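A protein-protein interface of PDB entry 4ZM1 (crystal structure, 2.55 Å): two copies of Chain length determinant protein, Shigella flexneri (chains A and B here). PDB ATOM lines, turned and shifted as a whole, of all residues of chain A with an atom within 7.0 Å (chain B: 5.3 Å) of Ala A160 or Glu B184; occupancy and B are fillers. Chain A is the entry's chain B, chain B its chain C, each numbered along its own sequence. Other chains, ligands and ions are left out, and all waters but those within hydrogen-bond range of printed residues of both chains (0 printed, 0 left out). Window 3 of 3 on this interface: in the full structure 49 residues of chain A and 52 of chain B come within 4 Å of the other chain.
The backbone carbonyl oxygen of Gln A155 lies within hydrogen-bond range of the side-chain hydroxyl of Ser B188 (3.3 Å). NE2 of Gln A159 sits at hydrogen-bond distance from O of Glu B184 (2.9 Å). OG of Ser B188 sits close to OE1 of Gln A159, 3.5 Å away.
The backbone carbonyl oxygen (O) of Ala A157 is in hydrogen-bond range of the backbone NH (N) of Val A162 (2.8 Å). O of Thr B163 sits at hydrogen-bond distance from N of Glu B184.
Among the printed residues, merely in contact across the chains: Phe A179 with Ala B185 (3.3 Å), Tyr A156 with Ser B188 (3.4 Å), Phe A179 with Pro B165 (3.5 Å), Gln A159 with Glu B187 (3.8 Å), Val A162 with Pro B165 (3.9 Å), Phe A179 with Gly B182 (3.95 Å) and Ala A160 with Glu B184 (3.99 Å).
Of the printed residues of chain B, Ala A160 touches Glu B184 (3.99 Å). Printed residues of chain A within 4 Å of Glu B184: Gln A159 and Ala A160. Printed residues of chain B within 4 Å of Gln A155: Ser B188. Of the printed residues of chain B, Phe A179 touches Pro B165, Gly B182 and Ala B185. Printed residues of chain B within 4 Å of Tyr A156: Ser B188 (3.4 Å). Of the printed residues of chain A, Pro B165 touches Val A162 and Phe A179. Of the printed residues of chain A, Ser B188 touches Gln A155, Tyr A156 and Gln A159. The nearest printed residue of chain B that does not touch Ala A160 is Lys B164 (4.3 Å). The nearest printed residue of chain A that does not touch Glu B184 is Gln A161 (5.3 Å). The nearest printed residue of chain A that does not touch Ala B185 is Tyr A156 (4.2 Å).
Of the 10 printed residues of chain A, 6 touch a printed residue of chain B. Hydrophobic or aromatic side chains of chain A that line the printed part of chain B: Tyr A156, Val A162 and Phe A179. Of the 11 printed residues of chain B, 6 touch a printed residue of chain A. Hydrophobic or aromatic side chains of chain B within 4 Å of the printed part of chain A: Pro B165 and Ala B185. Along chain B the printed residues that touch a printed residue of chain A span positions 165 to 188. Among the printed residues, no Asp or Glu carboxylate lies within 4 Å of a Lys or Arg side-chain nitrogen of the other chain.
2 positions are printed for both chains. Of the 10 pairs that touch across the chains among the printed residues, none has its exchanged pair printed and touching as well.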
ATOM      1  N   GLN A 155       3.318  10.865  -0.606  1.00  0.00           N
ATOM      2  CA  GLN A 155       3.325  10.996   0.851  1.00  0.00           C
ATOM      3  C   GLN A 155       2.078  10.345   1.419  1.00  0.00           C
ATOM      4  O   GLN A 155       2.172   9.674   2.434  1.00  0.00           O
ATOM      5  CB  GLN A 155       3.426  12.463   1.300  1.00  0.00           C
ATOM      6  CG  GLN A 155       4.656  13.182   0.730  1.00  0.00           C
ATOM      7  CD  GLN A 155       4.941  14.512   1.386  1.00  0.00           C
ATOM      8  OE1 GLN A 155       4.355  15.542   1.030  1.00  0.00           O
ATOM      9  NE2 GLN A 155       5.891  14.522   2.330  1.00  0.00           N
ATOM     10  N   TYR A 156       0.927  10.481   0.739  1.00  0.00           N
ATOM     11  CA  TYR A 156      -0.332   9.889   1.218  1.00  0.00           C
ATOM     12  C   TYR A 156      -0.308   8.373   1.101  1.00  0.00           C
ATOM     13  O   TYR A 156      -0.896   7.697   1.939  1.00  0.00           O
ATOM     14  CB  TYR A 156      -1.563  10.445   0.472  1.00  0.00           C
ATOM     15  CG  TYR A 156      -1.551  11.930   0.171  1.00  0.00           C
ATOM     16  CD1 TYR A 156      -0.990  12.841   1.063  1.00  0.00           C
ATOM     17  CD2 TYR A 156      -2.197  12.438  -0.956  1.00  0.00           C
ATOM     18  CE1 TYR A 156      -0.978  14.205   0.788  1.00  0.00           C
ATOM     19  CE2 TYR A 156      -2.214  13.803  -1.224  1.00  0.00           C
ATOM     20  CZ  TYR A 156      -1.609  14.684  -0.345  1.00  0.00           C
ATOM     21  OH  TYR A 156      -1.661  16.032  -0.573  1.00  0.00           O
ATOM     22  N   ALA A 157       0.329   7.848   0.033  1.00  0.00           N
ATOM     23  CA  ALA A 157       0.428   6.414  -0.225  1.00  0.00           C
ATOM     24  C   ALA A 157       1.412   5.760   0.743  1.00  0.00           C
ATOM     25  O   ALA A 157       1.183   4.625   1.159  1.00  0.00           O
ATOM     26  CB  ALA A 157       0.845   6.160  -1.672  1.00  0.00           C
ATOM     27  N   ASN A 158       2.486   6.465   1.118  1.00  0.00           N
ATOM     28  CA  ASN A 158       3.481   5.949   2.064  1.00  0.00           C
ATOM     29  C   ASN A 158       2.874   5.790   3.468  1.00  0.00           C
ATOM     30  O   ASN A 158       3.179   4.810   4.145  1.00  0.00           O
ATOM     31  CB  ASN A 158       4.702   6.856   2.125  1.00  0.00           C
ATOM     32  CG  ASN A 158       5.667   6.712   0.985  1.00  0.00           C
ATOM     33  OD1 ASN A 158       5.739   5.676   0.294  1.00  0.00           O
ATOM     34  ND2 ASN A 158       6.468   7.757   0.797  1.00  0.00           N
ATOM     35  N   GLN A 159       2.015   6.750   3.898  1.00  0.00           N
ATOM     36  CA  GLN A 159       1.349   6.684   5.193  1.00  0.00           C
ATOM     37  C   GLN A 159       0.293   5.570   5.194  1.00  0.00           C
ATOM     38  O   GLN A 159       0.284   4.786   6.145  1.00  0.00           O
ATOM     39  CB  GLN A 159       0.728   8.029   5.587  1.00  0.00           C
ATOM     40  CG  GLN A 159       0.680   8.214   7.116  1.00  0.00           C
ATOM     41  CD  GLN A 159      -0.053   9.459   7.572  1.00  0.00           C
ATOM     42  OE1 GLN A 159       0.407  10.599   7.375  1.00  0.00           O
ATOM     43  NE2 GLN A 159      -1.182   9.261   8.250  1.00  0.00           N
ATOM     44  N   ALA A 160      -0.551   5.448   4.120  1.00  0.00           N
ATOM     45  CA  ALA A 160      -1.584   4.396   4.034  1.00  0.00           C
ATOM     46  C   ALA A 160      -0.983   3.017   3.682  1.00  0.00           C
ATOM     47  O   ALA A 160      -1.691   2.003   3.713  1.00  0.00           O
ATOM     48  CB  ALA A 160      -2.642   4.768   3.020  1.00  0.00           C
ATOM     49  N   GLN A 161       0.338   2.985   3.386  1.00  0.00           N
ATOM     50  CA  GLN A 161       1.148   1.815   3.015  1.00  0.00           C
ATOM     51  C   GLN A 161       0.567   1.146   1.738  1.00  0.00           C
ATOM     52  O   GLN A 161       0.457  -0.074   1.632  1.00  0.00           O
ATOM     53  CB  GLN A 161       1.301   0.849   4.193  1.00  0.00           C
ATOM     54  CG  GLN A 161       1.805   1.537   5.460  1.00  0.00           C
ATOM     55  CD  GLN A 161       2.680   0.641   6.302  1.00  0.00           C
ATOM     56  OE1 GLN A 161       2.204  -0.162   7.116  1.00  0.00           O
ATOM     57  NE2 GLN A 161       3.984   0.772   6.127  1.00  0.00           N
ATOM     58  N   VAL A 162       0.191   1.998   0.772  1.00  0.00           N
ATOM     59  CA  VAL A 162      -0.371   1.633  -0.533  1.00  0.00           C
ATOM     60  C   VAL A 162       0.815   1.616  -1.507  1.00  0.00           C
ATOM     61  O   VAL A 162       1.363   2.670  -1.843  1.00  0.00           O
ATOM     62  CB  VAL A 162      -1.512   2.629  -0.906  1.00  0.00           C
ATOM     63  CG1 VAL A 162      -1.984   2.499  -2.359  1.00  0.00           C
ATOM     64  CG2 VAL A 162      -2.673   2.474   0.068  1.00  0.00           C
ATOM     65  N   THR A 163       1.265   0.413  -1.859  1.00  0.00           N
ATOM     66  CA  THR A 163       2.410   0.184  -2.744  1.00  0.00           C
ATOM     67  C   THR A 163       1.955  -0.210  -4.143  1.00  0.00           C
ATOM     68  O   THR A 163       2.493   0.307  -5.116  1.00  0.00           O
ATOM     69  CB  THR A 163       3.343  -0.899  -2.164  1.00  0.00           C
ATOM     70  OG1 THR A 163       2.546  -2.040  -1.842  1.00  0.00           O
ATOM     71  CG2 THR A 163       4.106  -0.421  -0.922  1.00  0.00           C
ATOM     72  N   PHE A 179      -2.995   8.839  -5.148  1.00  0.00           N
ATOM     73  CA  PHE A 179      -2.356   7.882  -4.244  1.00  0.00           C
ATOM     74  C   PHE A 179      -2.901   6.439  -4.402  1.00  0.00           C
ATOM     75  O   PHE A 179      -2.256   5.501  -3.936  1.00  0.00           O
ATOM     76  CB  PHE A 179      -2.480   8.360  -2.792  1.00  0.00           C
ATOM     77  CG  PHE A 179      -3.665   7.844  -2.004  1.00  0.00           C
ATOM     78  CD1 PHE A 179      -3.523   6.761  -1.129  1.00  0.00           C
ATOM     79  CD2 PHE A 179      -4.897   8.490  -2.064  1.00  0.00           C
ATOM     80  CE1 PHE A 179      -4.608   6.313  -0.363  1.00  0.00           C
ATOM     81  CE2 PHE A 179      -5.985   8.036  -1.301  1.00  0.00           C
ATOM     82  CZ  PHE A 179      -5.837   6.938  -0.475  1.00  0.00           C
ATOM     83  N   VAL B 162     -12.797   3.114   8.759  1.00  0.00           N
ATOM     84  CA  VAL B 162     -12.258   2.974   7.405  1.00  0.00           C
ATOM     85  C   VAL B 162     -10.866   3.608   7.449  1.00  0.00           C
ATOM     86  O   VAL B 162     -10.765   4.827   7.475  1.00  0.00           O
ATOM     87  CB  VAL B 162     -13.213   3.611   6.352  1.00  0.00           C
ATOM     88  CG1 VAL B 162     -12.632   3.521   4.932  1.00  0.00           C
ATOM     89  CG2 VAL B 162     -14.602   2.971   6.423  1.00  0.00           C
ATOM     90  N   THR B 163      -9.812   2.778   7.557  1.00  0.00           N
ATOM     91  CA  THR B 163      -8.414   3.206   7.713  1.00  0.00           C
ATOM     92  C   THR B 163      -7.649   3.102   6.412  1.00  0.00           C
ATOM     93  O   THR B 163      -6.876   4.009   6.101  1.00  0.00           O
ATOM     94  CB  THR B 163      -7.705   2.387   8.804  1.00  0.00           C
ATOM     95  OG1 THR B 163      -7.896   1.000   8.527  1.00  0.00           O
ATOM     96  CG2 THR B 163      -8.195   2.725  10.203  1.00  0.00           C
ATOM     97  N   LYS B 164      -7.802   1.970   5.699  1.00  0.00           N
ATOM     98  CA  LYS B 164      -7.171   1.721   4.402  1.00  0.00           C
ATOM     99  C   LYS B 164      -8.156   2.128   3.285  1.00  0.00           C
ATOM    100  O   LYS B 164      -9.357   2.131   3.558  1.00  0.00           O
ATOM    101  CB  LYS B 164      -6.774   0.237   4.281  1.00  0.00           C
ATOM    102  CG  LYS B 164      -5.477  -0.136   4.979  1.00  0.00           C
ATOM    103  CD  LYS B 164      -5.032  -1.525   4.532  1.00  0.00           C
ATOM    104  CE  LYS B 164      -3.539  -1.727   4.651  1.00  0.00           C
ATOM    105  NZ  LYS B 164      -3.137  -3.139   4.386  1.00  0.00           N
ATOM    106  N   PRO B 165      -7.718   2.456   2.036  1.00  0.00           N
ATOM    107  CA  PRO B 165      -8.690   2.832   0.993  1.00  0.00           C
ATOM    108  C   PRO B 165      -9.650   1.701   0.645  1.00  0.00           C
ATOM    109  O   PRO B 165      -9.263   0.526   0.632  1.00  0.00           O
ATOM    110  CB  PRO B 165      -7.813   3.189  -0.210  1.00  0.00           C
ATOM    111  CG  PRO B 165      -6.490   3.459   0.349  1.00  0.00           C
ATOM    112  CD  PRO B 165      -6.346   2.528   1.502  1.00  0.00           C
ATOM    113  N   GLY B 182      -8.266   6.234   2.562  1.00  0.00           N
ATOM    114  CA  GLY B 182      -7.888   5.847   3.926  1.00  0.00           C
ATOM    115  C   GLY B 182      -8.133   6.933   4.987  1.00  0.00           C
ATOM    116  O   GLY B 182      -8.047   8.122   4.675  1.00  0.00           O
ATOM    117  N   SER B 183      -8.424   6.566   6.257  1.00  0.00           N
ATOM    118  CA  SER B 183      -8.435   7.573   7.341  1.00  0.00           C
ATOM    119  C   SER B 183      -6.968   7.967   7.531  1.00  0.00           C
ATOM    120  O   SER B 183      -6.643   9.106   7.867  1.00  0.00           O
ATOM    121  CB  SER B 183      -9.057   7.043   8.634  1.00  0.00           C
ATOM    122  OG  SER B 183      -8.247   6.135   9.371  1.00  0.00           O
ATOM    123  N   GLU B 184      -6.088   6.979   7.256  1.00  0.00           N
ATOM    124  CA  GLU B 184      -4.641   7.080   7.209  1.00  0.00           C
ATOM    125  C   GLU B 184      -4.226   8.117   6.133  1.00  0.00           C
ATOM    126  O   GLU B 184      -3.452   9.040   6.434  1.00  0.00           O
ATOM    127  CB  GLU B 184      -4.046   5.694   6.888  1.00  0.00           C
ATOM    128  CG  GLU B 184      -4.012   4.722   8.046  1.00  0.00           C
ATOM    129  CD  GLU B 184      -2.662   4.655   8.745  1.00  0.00           C
ATOM    130  OE1 GLU B 184      -1.932   3.653   8.550  1.00  0.00           O
ATOM    131  OE2 GLU B 184      -2.321   5.624   9.464  1.00  0.00           O
ATOM    132  N   ALA B 185      -4.775   7.974   4.893  1.00  0.00           N
ATOM    133  CA  ALA B 185      -4.553   8.873   3.750  1.00  0.00           C
ATOM    134  C   ALA B 185      -5.111  10.262   3.993  1.00  0.00           C
ATOM    135  O   ALA B 185      -4.469  11.246   3.611  1.00  0.00           O
ATOM    136  CB  ALA B 185      -5.205   8.304   2.516  1.00  0.00           C
ATOM    137  N   LEU B 186      -6.326  10.354   4.576  1.00  0.00           N
ATOM    138  CA  LEU B 186      -6.963  11.656   4.855  1.00  0.00           C
ATOM    139  C   LEU B 186      -6.148  12.432   5.921  1.00  0.00           C
ATOM    140  O   LEU B 186      -6.001  13.648   5.796  1.00  0.00           O
ATOM    141  CB  LEU B 186      -8.455  11.526   5.263  1.00  0.00           C
ATOM    142  CG  LEU B 186      -9.415  10.792   4.296  1.00  0.00           C
ATOM    143  CD1 LEU B 186     -10.708  10.417   4.986  1.00  0.00           C
ATOM    144  CD2 LEU B 186      -9.726  11.605   3.080  1.00  0.00           C
ATOM    145  N   GLU B 187      -5.576  11.734   6.924  1.00  0.00           N
ATOM    146  CA  GLU B 187      -4.712  12.363   7.939  1.00  0.00           C
ATOM    147  C   GLU B 187      -3.484  12.946   7.252  1.00  0.00           C
ATOM    148  O   GLU B 187      -3.096  14.077   7.553  1.00  0.00           O
ATOM    149  CB  GLU B 187      -4.288  11.351   9.022  1.00  0.00           C
ATOM    150  CG  GLU B 187      -5.143  11.360  10.270  1.00  0.00           C
ATOM    151  CD  GLU B 187      -5.075  10.109  11.133  1.00  0.00           C
ATOM    152  OE1 GLU B 187      -3.985   9.500  11.260  1.00  0.00           O
ATOM    153  OE2 GLU B 187      -6.135   9.737  11.687  1.00  0.00           O
ATOM    154  N   SER B 188      -2.901  12.180   6.292  1.00  0.00           N
ATOM    155  CA  SER B 188      -1.721  12.547   5.512  1.00  0.00           C
ATOM    156  C   SER B 188      -1.984  13.802   4.675  1.00  0.00           C
ATOM    157  O   SER B 188      -1.109  14.662   4.547  1.00  0.00           O
ATOM    158  CB  SER B 188      -1.309  11.391   4.614  1.00  0.00           C
ATOM    159  OG  SER B 188      -0.009  11.598   4.093  1.00  0.00           O
